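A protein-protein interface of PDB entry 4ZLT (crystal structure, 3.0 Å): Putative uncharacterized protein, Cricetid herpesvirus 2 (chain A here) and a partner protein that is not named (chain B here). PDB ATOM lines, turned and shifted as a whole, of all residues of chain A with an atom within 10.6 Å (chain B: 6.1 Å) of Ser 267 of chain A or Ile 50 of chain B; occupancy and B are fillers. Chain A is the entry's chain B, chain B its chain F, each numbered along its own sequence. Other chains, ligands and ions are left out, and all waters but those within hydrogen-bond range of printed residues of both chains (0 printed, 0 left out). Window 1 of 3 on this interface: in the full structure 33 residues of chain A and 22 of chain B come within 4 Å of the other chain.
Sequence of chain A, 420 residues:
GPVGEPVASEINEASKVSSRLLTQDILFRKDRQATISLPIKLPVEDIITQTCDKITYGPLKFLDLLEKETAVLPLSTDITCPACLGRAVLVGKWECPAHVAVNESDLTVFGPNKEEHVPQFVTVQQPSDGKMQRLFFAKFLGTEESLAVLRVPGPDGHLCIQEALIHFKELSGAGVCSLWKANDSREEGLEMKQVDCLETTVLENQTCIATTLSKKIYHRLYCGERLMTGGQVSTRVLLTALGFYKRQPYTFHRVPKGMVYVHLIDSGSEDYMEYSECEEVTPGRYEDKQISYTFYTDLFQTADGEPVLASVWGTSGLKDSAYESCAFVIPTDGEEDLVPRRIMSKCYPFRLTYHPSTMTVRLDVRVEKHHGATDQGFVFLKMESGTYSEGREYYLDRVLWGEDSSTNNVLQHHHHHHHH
The backbone NH (N) of Gly 268 of chain A is in hydrogen-bond range of the side-chain hydroxyl (OG) of Ser 15 of chain B, 3.1 Å away. The side-chain hydroxyl of Ser 267 of chain A sits at hydrogen-bond distance from the backbone NH of Cys 51 of chain B, 3.1 Å away. O of Tyr 16 of chain B sits close to N of Gly 268 of chain A (3.4 Å). N of Ser 15 of chain B lies within hydrogen-bond range of O of Ile 265 of chain A, 3.3 Å away. OD1 of Asp 266 of chain A is in hydrogen-bond range of OG of Ser 15 of chain B (2.4 Å). The side-chain hydroxyl (OG) of Ser 15 of chain B is in hydrogen-bond range of the backbone NH (N) of Ser 267 of chain A (3.0 Å). O of Ile 265 of chain A is in hydrogen-bond range of N of Phe 14 of chain B (2.8 Å).
N of Leu 264 of chain A lies within hydrogen-bond range of O of Leu 239 of chain A (3.0 Å). The backbone NH (N) of Phe 42 of chain B is in hydrogen-bond range of the backbone carbonyl oxygen (O) of Ile 50 of chain B (2.8 Å). OG1 of Thr 44 of chain B sits at hydrogen-bond distance from O of Arg 48 of chain B (3.2 Å). N of Ser 17 of chain B is in hydrogen-bond range of O of Cys 51 of chain B (2.9 Å). The side-chain carboxylate of Asp 266 of chain A is in hydrogen-bond range of the side-chain hydroxyl of Ser 269 of chain A.
Thr 200 of chain A touches Phe 14 of chain B. Phe 14 of chain B touches Leu 239 of chain A. CD1 of Leu 264 of chain A touches CD1 of Phe 14 of chain B (3.8 Å). C of Cys 13 of chain B touches O of Ile 265 of chain A, at 3.7 Å. OE1 of Gln 49 of chain B touches CD1 of Ile 265 of chain A, 3.5 Å away. Cys 51 of chain B touches Ile 265 of chain A. Asp 266 of chain A touches Phe 14 of chain B (OD1 to CD2, 3.8 Å). O of Ser 267 of chain A touches CB of Ser 17 of chain B, at 3.7 Å. OG of Ser 267 of chain A touches CA of Ile 50 of chain B (3.9 Å). CB of Thr 44 of chain B touches OH of Tyr 272 of chain A (3.5 Å).
Of the printed residues of chain B, Ser 267 of chain A touches Ser 15, Tyr 16, Ser 17, Ile 50 and Cys 51. Glu 270 of chain A touches none of the printed residues of chain B. Of the printed residues of chain B, Tyr 272 of chain A touches Thr 44 (3.5 Å). Of the printed residues of chain A, Phe 14 of chain B touches Thr 200, Leu 239, Leu 264, Ile 265 and Asp 266. Ser 15 of chain B touches just these residues of chain A: Ile 265, Asp 266, Ser 267 and Gly 268. Ser 17 of chain B touches one residue of chain A. No residue of chain A comes within 4 Å of Ile 41 of chain B. Of the printed residues of chain A, Gln 49 of chain B touches Ile 265 (3.5 Å). Printed residues of chain A within 4 Å of Ile 50 of chain B: Ser 267. Of chain A, only Ile 265 and Ser 267 come within 4 Å of Cys 51 of chain B. The nearest printed residue of chain B that does not touch Asp 271 of chain A is Ser 17 of chain B (5.9 Å).
Of the 18 printed residues of chain A, 9 touch a printed residue of chain B. Printed residues of chain A that touch a printed residue of chain B: Thr 200, Leu 239, Leu 264, Ile 265, Asp 266, Ser 267, Gly 268, Asp 271 and Tyr 272. Of the 18 printed residues of chain B, 10 touch a printed residue of chain A. Hydrophobic or aromatic side chains of chain B that line the printed part of chain A: Phe 14. Among the printed residues, 20 pairs touch across the chains.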
ATOM      1  N   PRO A  82      10.465  17.521  20.916  1.00  0.00           N
ATOM      2  CA  PRO A  82      11.338  18.680  21.156  1.00  0.00           C
ATOM      3  C   PRO A  82      10.720  19.734  22.051  1.00  0.00           C
ATOM      4  O   PRO A  82      11.451  20.425  22.768  1.00  0.00           O
ATOM      5  CB  PRO A  82      11.602  19.215  19.742  1.00  0.00           C
ATOM      6  CG  PRO A  82      10.467  18.704  18.921  1.00  0.00           C
ATOM      7  CD  PRO A  82      10.122  17.366  19.494  1.00  0.00           C
ATOM      8  N   GLU A 145      14.907  20.250  24.230  1.00  0.00           N
ATOM      9  CA  GLU A 145      15.983  20.929  23.524  1.00  0.00           C
ATOM     10  C   GLU A 145      16.877  21.740  24.450  1.00  0.00           C
ATOM     11  O   GLU A 145      17.721  22.502  23.968  1.00  0.00           O
ATOM     12  CB  GLU A 145      15.412  21.845  22.442  1.00  0.00           C
ATOM     13  CG  GLU A 145      14.851  21.121  21.238  1.00  0.00           C
ATOM     14  CD  GLU A 145      14.434  22.077  20.141  1.00  0.00           C
ATOM     15  OE1 GLU A 145      13.997  23.199  20.470  1.00  0.00           O
ATOM     16  OE2 GLU A 145      14.550  21.711  18.953  1.00  0.00           O
ATOM     17  N   THR A 200      24.022  37.015  15.142  1.00  0.00           N
ATOM     18  CA  THR A 200      22.626  36.608  15.239  1.00  0.00           C
ATOM     19  C   THR A 200      22.007  37.075  16.549  1.00  0.00           C
ATOM     20  O   THR A 200      20.847  37.496  16.579  1.00  0.00           O
ATOM     21  CB  THR A 200      22.506  35.090  15.108  1.00  0.00           C
ATOM     22  OG1 THR A 200      22.901  34.687  13.792  1.00  0.00           O
ATOM     23  CG2 THR A 200      21.077  34.650  15.359  1.00  0.00           C
ATOM     24  N   VAL A 237      22.740  18.184  15.331  1.00  0.00           N
ATOM     25  CA  VAL A 237      23.669  19.306  15.403  1.00  0.00           C
ATOM     26  C   VAL A 237      23.054  20.375  16.290  1.00  0.00           C
ATOM     27  O   VAL A 237      21.936  20.836  16.037  1.00  0.00           O
ATOM     28  CB  VAL A 237      23.995  19.867  14.012  1.00  0.00           C
ATOM     29  CG1 VAL A 237      25.097  20.908  14.112  1.00  0.00           C
ATOM     30  CG2 VAL A 237      24.394  18.748  13.074  1.00  0.00           C
ATOM     31  N   LEU A 239      23.481  24.094  17.484  1.00  0.00           N
ATOM     32  CA  LEU A 239      24.101  25.395  17.271  1.00  0.00           C
ATOM     33  C   LEU A 239      23.687  26.302  18.424  1.00  0.00           C
ATOM     34  O   LEU A 239      22.521  26.693  18.526  1.00  0.00           O
ATOM     35  CB  LEU A 239      23.686  25.973  15.924  1.00  0.00           C
ATOM     36  CG  LEU A 239      24.474  27.187  15.447  1.00  0.00           C
ATOM     37  CD1 LEU A 239      25.951  26.858  15.397  1.00  0.00           C
ATOM     38  CD2 LEU A 239      23.972  27.622  14.086  1.00  0.00           C
ATOM     39  N   HIS A 263      19.570  29.280  21.996  1.00  0.00           N
ATOM     40  CA  HIS A 263      19.439  28.311  20.918  1.00  0.00           C
ATOM     41  C   HIS A 263      19.405  29.023  19.573  1.00  0.00           C
ATOM     42  O   HIS A 263      18.681  30.007  19.399  1.00  0.00           O
ATOM     43  CB  HIS A 263      18.169  27.486  21.122  1.00  0.00           C
ATOM     44  CG  HIS A 263      18.077  26.283  20.238  1.00  0.00           C
ATOM     45  ND1 HIS A 263      16.880  25.668  19.943  1.00  0.00           N
ATOM     46  CD2 HIS A 263      19.035  25.573  19.595  1.00  0.00           C
ATOM     47  CE1 HIS A 263      17.103  24.635  19.151  1.00  0.00           C
ATOM     48  NE2 HIS A 263      18.403  24.555  18.924  1.00  0.00           N
ATOM     49  N   LEU A 264      20.192  28.531  18.622  1.00  0.00           N
ATOM     50  CA  LEU A 264      20.230  29.065  17.267  1.00  0.00           C
ATOM     51  C   LEU A 264      19.689  28.017  16.304  1.00  0.00           C
ATOM     52  O   LEU A 264      20.105  26.856  16.345  1.00  0.00           O
ATOM     53  CB  LEU A 264      21.649  29.474  16.872  1.00  0.00           C
ATOM     54  CG  LEU A 264      22.257  30.636  17.661  1.00  0.00           C
ATOM     55  CD1 LEU A 264      23.695  30.889  17.245  1.00  0.00           C
ATOM     56  CD2 LEU A 264      21.430  31.882  17.475  1.00  0.00           C
ATOM     57  N   ILE A 265      18.763  28.431  15.446  1.00  0.00           N
ATOM     58  CA  ILE A 265      18.058  27.536  14.538  1.00  0.00           C
ATOM     59  C   ILE A 265      18.572  27.796  13.130  1.00  0.00           C
ATOM     60  O   ILE A 265      18.295  28.849  12.542  1.00  0.00           O
ATOM     61  CB  ILE A 265      16.539  27.732  14.615  1.00  0.00           C
ATOM     62  CG1 ILE A 265      16.046  27.472  16.038  1.00  0.00           C
ATOM     63  CG2 ILE A 265      15.832  26.829  13.615  1.00  0.00           C
ATOM     64  CD1 ILE A 265      14.572  27.702  16.220  1.00  0.00           C
ATOM     65  N   ASP A 266      19.320  26.838  12.589  1.00  0.00           N
ATOM     66  CA  ASP A 266      19.816  26.887  11.216  1.00  0.00           C
ATOM     67  C   ASP A 266      18.869  26.059  10.359  1.00  0.00           C
ATOM     68  O   ASP A 266      18.985  24.833  10.297  1.00  0.00           O
ATOM     69  CB  ASP A 266      21.246  26.368  11.141  1.00  0.00           C
ATOM     70  CG  ASP A 266      21.773  26.313   9.726  1.00  0.00           C
ATOM     71  OD1 ASP A 266      22.124  27.380   9.181  1.00  0.00           O
ATOM     72  OD2 ASP A 266      21.841  25.203   9.158  1.00  0.00           O
ATOM     73  N   SER A 267      17.927  26.728   9.701  1.00  0.00           N
ATOM     74  CA  SER A 267      16.892  26.045   8.939  1.00  0.00           C
ATOM     75  C   SER A 267      17.162  26.009   7.442  1.00  0.00           C
ATOM     76  O   SER A 267      16.407  25.359   6.712  1.00  0.00           O
ATOM     77  CB  SER A 267      15.530  26.704   9.191  1.00  0.00           C
ATOM     78  OG  SER A 267      15.099  26.479  10.521  1.00  0.00           O
ATOM     79  N   GLY A 268      18.212  26.679   6.968  1.00  0.00           N
ATOM     80  CA  GLY A 268      18.505  26.670   5.547  1.00  0.00           C
ATOM     81  C   GLY A 268      18.917  25.316   5.013  1.00  0.00           C
ATOM     82  O   GLY A 268      18.911  25.111   3.795  1.00  0.00           O
ATOM     83  N   SER A 269      19.256  24.377   5.895  1.00  0.00           N
ATOM     84  CA  SER A 269      19.833  23.116   5.443  1.00  0.00           C
ATOM     85  C   SER A 269      18.784  22.155   4.897  1.00  0.00           C
ATOM     86  O   SER A 269      19.036  21.461   3.907  1.00  0.00           O
ATOM     87  CB  SER A 269      20.604  22.457   6.588  1.00  0.00           C
ATOM     88  OG  SER A 269      21.716  23.247   6.965  1.00  0.00           O
ATOM     89  N   GLU A 270      17.611  22.095   5.516  1.00  0.00           N
ATOM     90  CA  GLU A 270      16.659  21.030   5.236  1.00  0.00           C
ATOM     91  C   GLU A 270      15.504  21.511   4.362  1.00  0.00           C
ATOM     92  O   GLU A 270      15.268  22.710   4.192  1.00  0.00           O
ATOM     93  CB  GLU A 270      16.114  20.440   6.540  1.00  0.00           C
ATOM     94  CG  GLU A 270      15.310  19.163   6.344  1.00  0.00           C
ATOM     95  CD  GLU A 270      14.493  18.781   7.561  1.00  0.00           C
ATOM     96  OE1 GLU A 270      14.764  17.714   8.150  1.00  0.00           O
ATOM     97  OE2 GLU A 270      13.579  19.550   7.931  1.00  0.00           O
ATOM     98  N   ASP A 271      14.787  20.538   3.800  1.00  0.00           N
ATOM     99  CA  ASP A 271      13.577  20.758   3.024  1.00  0.00           C
ATOM    100  C   ASP A 271      12.480  19.840   3.549  1.00  0.00           C
ATOM    101  O   ASP A 271      12.733  18.896   4.301  1.00  0.00           O
ATOM    102  CB  ASP A 271      13.805  20.501   1.527  1.00  0.00           C
ATOM    103  CG  ASP A 271      14.808  21.455   0.914  1.00  0.00           C
ATOM    104  OD1 ASP A 271      14.966  22.577   1.439  1.00  0.00           O
ATOM    105  OD2 ASP A 271      15.434  21.085  -0.100  1.00  0.00           O
ATOM    106  N   TYR A 272      11.245  20.120   3.131  1.00  0.00           N
ATOM    107  CA  TYR A 272      10.082  19.355   3.565  1.00  0.00           C
ATOM    108  C   TYR A 272       9.729  18.227   2.601  1.00  0.00           C
ATOM    109  O   TYR A 272       8.553  17.855   2.490  1.00  0.00           O
ATOM    110  CB  TYR A 272       8.885  20.287   3.755  1.00  0.00           C
ATOM    111  CG  TYR A 272       8.111  20.039   5.032  1.00  0.00           C
ATOM    112  CD1 TYR A 272       7.315  18.912   5.177  1.00  0.00           C
ATOM    113  CD2 TYR A 272       8.173  20.936   6.090  1.00  0.00           C
ATOM    114  CE1 TYR A 272       6.610  18.682   6.339  1.00  0.00           C
ATOM    115  CE2 TYR A 272       7.467  20.711   7.257  1.00  0.00           C
ATOM    116  CZ  TYR A 272       6.688  19.583   7.374  1.00  0.00           C
ATOM    117  OH  TYR A 272       5.981  19.347   8.527  1.00  0.00           O
ATOM    118  N   MET A 273      10.719  17.665   1.906  1.00  0.00           N
ATOM    119  CA  MET A 273      10.421  16.679   0.872  1.00  0.00           C
ATOM    120  C   MET A 273       9.912  15.370   1.458  1.00  0.00           C
ATOM    121  O   MET A 273       9.100  14.686   0.825  1.00  0.00           O
ATOM    122  CB  MET A 273      11.661  16.428   0.013  1.00  0.00           C
ATOM    123  CG  MET A 273      12.041  17.601  -0.872  1.00  0.00           C
ATOM    124  SD  MET A 273      10.704  18.048  -1.995  1.00  0.00           S
ATOM    125  CE  MET A 273      11.408  19.466  -2.832  1.00  0.00           C
ATOM    126  N   GLU A 274      10.370  15.003   2.656  1.00  0.00           N
ATOM    127  CA  GLU A 274       9.972  13.722   3.231  1.00  0.00           C
ATOM    128  C   GLU A 274       8.462  13.643   3.420  1.00  0.00           C
ATOM    129  O   GLU A 274       7.850  12.602   3.150  1.00  0.00           O
ATOM    130  CB  GLU A 274      10.704  13.491   4.553  1.00  0.00           C
ATOM    131  CG  GLU A 274      11.014  14.757   5.336  1.00  0.00           C
ATOM    132  CD  GLU A 274      11.885  14.490   6.550  1.00  0.00           C
ATOM    133  OE1 GLU A 274      12.039  13.310   6.924  1.00  0.00           O
ATOM    134  OE2 GLU A 274      12.422  15.458   7.128  1.00  0.00           O
ATOM    135  N   TYR A 275       7.843  14.729   3.874  1.00  0.00           N
ATOM    136  CA  TYR A 275       6.397  14.767   4.043  1.00  0.00           C
ATOM    137  C   TYR A 275       5.661  15.089   2.748  1.00  0.00           C
ATOM    138  O   TYR A 275       4.428  15.030   2.724  1.00  0.00           O
ATOM    139  CB  TYR A 275       6.024  15.783   5.131  1.00  0.00           C
ATOM    140  CG  TYR A 275       4.536  15.926   5.378  1.00  0.00           C
ATOM    141  CD1 TYR A 275       3.742  14.816   5.630  1.00  0.00           C
ATOM    142  CD2 TYR A 275       3.926  17.174   5.368  1.00  0.00           C
ATOM    143  CE1 TYR A 275       2.381  14.943   5.856  1.00  0.00           C
ATOM    144  CE2 TYR A 275       2.568  17.311   5.596  1.00  0.00           C
ATOM    145  CZ  TYR A 275       1.801  16.194   5.839  1.00  0.00           C
ATOM    146  OH  TYR A 275       0.448  16.327   6.064  1.00  0.00           O
ATOM    147  N   CYS B  13      16.963  32.858  14.992  1.00  0.00           N
ATOM    148  CA  CYS B  13      17.120  32.299  13.652  1.00  0.00           C
ATOM    149  C   CYS B  13      18.545  32.512  13.153  1.00  0.00           C
ATOM    150  O   CYS B  13      18.950  33.645  12.881  1.00  0.00           O
ATOM    151  CB  CYS B  13      16.115  32.930  12.695  1.00  0.00           C
ATOM    152  SG  CYS B  13      14.429  32.424  13.003  1.00  0.00           S
ATOM    153  N   PHE B  14      19.303  31.423  13.024  1.00  0.00           N
ATOM    154  CA  PHE B  14      20.643  31.500  12.456  1.00  0.00           C
ATOM    155  C   PHE B  14      20.640  31.482  10.935  1.00  0.00           C
ATOM    156  O   PHE B  14      21.592  31.972  10.318  1.00  0.00           O
ATOM    157  CB  PHE B  14      21.500  30.342  12.969  1.00  0.00           C
ATOM    158  CG  PHE B  14      22.966  30.508  12.698  1.00  0.00           C
ATOM    159  CD1 PHE B  14      23.751  31.306  13.507  1.00  0.00           C
ATOM    160  CD2 PHE B  14      23.557  29.865  11.626  1.00  0.00           C
ATOM    161  CE1 PHE B  14      25.099  31.456  13.251  1.00  0.00           C
ATOM    162  CE2 PHE B  14      24.901  30.011  11.368  1.00  0.00           C
ATOM    163  CZ  PHE B  14      25.671  30.806  12.180  1.00  0.00           C
ATOM    164  N   SER B  15      19.594  30.940  10.321  1.00  0.00           N
ATOM    165  CA  SER B  15      19.475  30.906   8.873  1.00  0.00           C
ATOM    166  C   SER B  15      18.025  30.621   8.527  1.00  0.00           C
ATOM    167  O   SER B  15      17.358  29.855   9.223  1.00  0.00           O
ATOM    168  CB  SER B  15      20.396  29.845   8.266  1.00  0.00           C
ATOM    169  OG  SER B  15      20.028  28.549   8.702  1.00  0.00           O
ATOM    170  N   TYR B  16      17.552  31.224   7.446  1.00  0.00           N
ATOM    171  CA  TYR B  16      16.148  31.132   7.085  1.00  0.00           C
ATOM    172  C   TYR B  16      15.908  29.971   6.128  1.00  0.00           C
ATOM    173  O   TYR B  16      16.827  29.456   5.489  1.00  0.00           O
ATOM    174  CB  TYR B  16      15.678  32.448   6.472  1.00  0.00           C
ATOM    175  CG  TYR B  16      15.846  33.613   7.420  1.00  0.00           C
ATOM    176  CD1 TYR B  16      15.190  33.637   8.641  1.00  0.00           C
ATOM    177  CD2 TYR B  16      16.667  34.681   7.100  1.00  0.00           C
ATOM    178  CE1 TYR B  16      15.343  34.692   9.514  1.00  0.00           C
ATOM    179  CE2 TYR B  16      16.826  35.743   7.967  1.00  0.00           C
ATOM    180  CZ  TYR B  16      16.160  35.743   9.172  1.00  0.00           C
ATOM    181  OH  TYR B  16      16.314  36.800  10.038  1.00  0.00           O
ATOM    182  N   SER B  17      14.649  29.558   6.041  1.00  0.00           N
ATOM    183  CA  SER B  17      14.264  28.354   5.326  1.00  0.00           C
ATOM    184  C   SER B  17      13.545  28.708   4.032  1.00  0.00           C
ATOM    185  O   SER B  17      13.040  29.820   3.854  1.00  0.00           O
ATOM    186  CB  SER B  17      13.368  27.463   6.190  1.00  0.00           C
ATOM    187  OG  SER B  17      12.818  26.405   5.428  1.00  0.00           O
ATOM    188  N   ARG B  18      13.507  27.738   3.124  1.00  0.00           N
ATOM    189  CA  ARG B  18      12.800  27.923   1.869  1.00  0.00           C
ATOM    190  C   ARG B  18      11.295  27.884   2.095  1.00  0.00           C
ATOM    191  O   ARG B  18      10.801  27.282   3.051  1.00  0.00           O
ATOM    192  CB  ARG B  18      13.204  26.844   0.863  1.00  0.00           C
ATOM    193  CG  ARG B  18      12.539  25.494   1.097  1.00  0.00           C
ATOM    194  CD  ARG B  18      12.950  24.480   0.040  1.00  0.00           C
ATOM    195  NE  ARG B  18      12.968  25.058  -1.303  1.00  0.00           N
ATOM    196  CZ  ARG B  18      11.903  25.167  -2.090  1.00  0.00           C
ATOM    197  NH1 ARG B  18      10.717  24.741  -1.672  1.00  0.00           N
ATOM    198  NH2 ARG B  18      12.021  25.706  -3.297  1.00  0.00           N
ATOM    199  N   ILE B  20       7.478  26.888   1.939  1.00  0.00           N
ATOM    200  CA  ILE B  20       6.826  25.578   1.949  1.00  0.00           C
ATOM    201  C   ILE B  20       5.325  25.774   1.848  1.00  0.00           C
ATOM    202  O   ILE B  20       4.782  26.817   2.223  1.00  0.00           O
ATOM    203  CB  ILE B  20       7.161  24.773   3.218  1.00  0.00           C
ATOM    204  CG1 ILE B  20       6.668  25.502   4.464  1.00  0.00           C
ATOM    205  CG2 ILE B  20       8.657  24.540   3.311  1.00  0.00           C
ATOM    206  CD1 ILE B  20       7.037  24.806   5.750  1.00  0.00           C
ATOM    207  N   ILE B  25       1.934  24.618   7.540  1.00  0.00           N
ATOM    208  CA  ILE B  25       2.138  25.508   8.677  1.00  0.00           C
ATOM    209  C   ILE B  25       0.885  25.500   9.540  1.00  0.00           C
ATOM    210  O   ILE B  25      -0.235  25.600   9.025  1.00  0.00           O
ATOM    211  CB  ILE B  25       2.471  26.932   8.204  1.00  0.00           C
ATOM    212  CG1 ILE B  25       3.769  26.933   7.398  1.00  0.00           C
ATOM    213  CG2 ILE B  25       2.578  27.872   9.391  1.00  0.00           C
ATOM    214  CD1 ILE B  25       4.961  26.432   8.173  1.00  0.00           C
ATOM    215  N   VAL B  40      10.868  35.005  11.933  1.00  0.00           N
ATOM    216  CA  VAL B  40       9.616  34.307  12.193  1.00  0.00           C
ATOM    217  C   VAL B  40       9.924  32.831  12.374  1.00  0.00           C
ATOM    218  O   VAL B  40      10.752  32.266  11.653  1.00  0.00           O
ATOM    219  CB  VAL B  40       8.598  34.520  11.057  1.00  0.00           C
ATOM    220  CG1 VAL B  40       7.362  33.679  11.296  1.00  0.00           C
ATOM    221  CG2 VAL B  40       8.229  35.987  10.950  1.00  0.00           C
ATOM    222  N   ILE B  41       9.270  32.211  13.347  1.00  0.00           N
ATOM    223  CA  ILE B  41       9.429  30.793  13.627  1.00  0.00           C
ATOM    224  C   ILE B  41       8.085  30.128  13.382  1.00  0.00           C
ATOM    225  O   ILE B  41       7.153  30.289  14.179  1.00  0.00           O
ATOM    226  CB  ILE B  41       9.915  30.541  15.058  1.00  0.00           C
ATOM    227  CG1 ILE B  41      11.219  31.293  15.314  1.00  0.00           C
ATOM    228  CG2 ILE B  41      10.094  29.053  15.305  1.00  0.00           C
ATOM    229  CD1 ILE B  41      11.767  31.095  16.698  1.00  0.00           C
ATOM    230  N   PHE B  42       7.977  29.389  12.284  1.00  0.00           N
ATOM    231  CA  PHE B  42       6.756  28.661  11.988  1.00  0.00           C
ATOM    232  C   PHE B  42       6.747  27.325  12.717  1.00  0.00           C
ATOM    233  O   PHE B  42       7.776  26.653  12.825  1.00  0.00           O
ATOM    234  CB  PHE B  42       6.620  28.425  10.485  1.00  0.00           C
ATOM    235  CG  PHE B  42       6.277  29.659   9.703  1.00  0.00           C
ATOM    236  CD1 PHE B  42       5.088  30.330   9.928  1.00  0.00           C
ATOM    237  CD2 PHE B  42       7.138  30.142   8.735  1.00  0.00           C
ATOM    238  CE1 PHE B  42       4.771  31.462   9.209  1.00  0.00           C
ATOM    239  CE2 PHE B  42       6.825  31.272   8.012  1.00  0.00           C
ATOM    240  CZ  PHE B  42       5.639  31.934   8.251  1.00  0.00           C
ATOM    241  N   LEU B  43       5.585  26.953  13.241  1.00  0.00           N
ATOM    242  CA  LEU B  43       5.373  25.629  13.806  1.00  0.00           C
ATOM    243  C   LEU B  43       4.584  24.797  12.804  1.00  0.00           C
ATOM    244  O   LEU B  43       3.529  25.227  12.329  1.00  0.00           O
ATOM    245  CB  LEU B  43       4.635  25.709  15.143  1.00  0.00           C
ATOM    246  CG  LEU B  43       4.509  24.393  15.912  1.00  0.00           C
ATOM    247  CD1 LEU B  43       5.865  23.953  16.437  1.00  0.00           C
ATOM    248  CD2 LEU B  43       3.513  24.525  17.051  1.00  0.00           C
ATOM    249  N   THR B  44       5.094  23.618  12.481  1.00  0.00           N
ATOM    250  CA  THR B  44       4.511  22.789  11.438  1.00  0.00           C
ATOM    251  C   THR B  44       3.597  21.727  12.034  1.00  0.00           C
ATOM    252  O   THR B  44       3.603  21.464  13.238  1.00  0.00           O
ATOM    253  CB  THR B  44       5.610  22.131  10.603  1.00  0.00           C
ATOM    254  OG1 THR B  44       6.405  21.289  11.445  1.00  0.00           O
ATOM    255  CG2 THR B  44       6.493  23.189   9.967  1.00  0.00           C
ATOM    256  N   ARG B  48       7.388  20.717  14.552  1.00  0.00           N
ATOM    257  CA  ARG B  48       8.770  21.157  14.453  1.00  0.00           C
ATOM    258  C   ARG B  48       8.823  22.639  14.105  1.00  0.00           C
ATOM    259  O   ARG B  48       7.897  23.184  13.495  1.00  0.00           O
ATOM    260  CB  ARG B  48       9.532  20.345  13.401  1.00  0.00           C
ATOM    261  CG  ARG B  48       9.796  18.900  13.805  1.00  0.00           C
ATOM    262  CD  ARG B  48      10.753  18.213  12.839  1.00  0.00           C
ATOM    263  NE  ARG B  48      10.859  16.779  13.097  1.00  0.00           N
ATOM    264  CZ  ARG B  48      11.667  16.237  14.003  1.00  0.00           C
ATOM    265  NH1 ARG B  48      12.447  17.009  14.749  1.00  0.00           N
ATOM    266  NH2 ARG B  48      11.696  14.921  14.165  1.00  0.00           N
ATOM    267  N   GLN B  49       9.919  23.284  14.492  1.00  0.00           N
ATOM    268  CA  GLN B  49      10.100  24.711  14.276  1.00  0.00           C
ATOM    269  C   GLN B  49      10.899  24.945  13.000  1.00  0.00           C
ATOM    270  O   GLN B  49      11.807  24.178  12.672  1.00  0.00           O
ATOM    271  CB  GLN B  49      10.803  25.364  15.467  1.00  0.00           C
ATOM    272  CG  GLN B  49      10.026  25.260  16.770  1.00  0.00           C
ATOM    273  CD  GLN B  49      10.777  25.839  17.953  1.00  0.00           C
ATOM    274  OE1 GLN B  49      11.980  26.078  17.886  1.00  0.00           O
ATOM    275  NE2 GLN B  49      10.067  26.062  19.051  1.00  0.00           N
ATOM    276  N   ILE B  50      10.555  26.016  12.289  1.00  0.00           N
ATOM    277  CA  ILE B  50      11.192  26.374  11.028  1.00  0.00           C
ATOM    278  C   ILE B  50      11.374  27.883  11.000  1.00  0.00           C
ATOM    279  O   ILE B  50      10.402  28.629  11.163  1.00  0.00           O
ATOM    280  CB  ILE B  50      10.369  25.915   9.817  1.00  0.00           C
ATOM    281  CG1 ILE B  50      10.379  24.392   9.720  1.00  0.00           C
ATOM    282  CG2 ILE B  50      10.896  26.553   8.549  1.00  0.00           C
ATOM    283  CD1 ILE B  50       9.599  23.854   8.547  1.00  0.00           C
ATOM    284  N   CYS B  51      12.604  28.334  10.800  1.00  0.00           N
ATOM    285  CA  CYS B  51      12.897  29.756  10.737  1.00  0.00           C
ATOM    286  C   CYS B  51      12.665  30.277   9.325  1.00  0.00           C
ATOM    287  O   CYS B  51      12.923  29.579   8.342  1.00  0.00           O
ATOM    288  CB  CYS B  51      14.334  30.028  11.173  1.00  0.00           C
ATOM    289  SG  CYS B  51      14.501  30.402  12.923  1.00  0.00           S
ATOM    290  N   ALA B  52      12.153  31.500   9.232  1.00  0.00           N
ATOM    291  CA  ALA B  52      11.893  32.126   7.946  1.00  0.00           C
ATOM    292  C   ALA B  52      12.092  33.628   8.080  1.00  0.00           C
ATOM    293  O   ALA B  52      11.901  34.199   9.157  1.00  0.00           O
ATOM    294  CB  ALA B  52      10.479  31.814   7.447  1.00  0.00           C
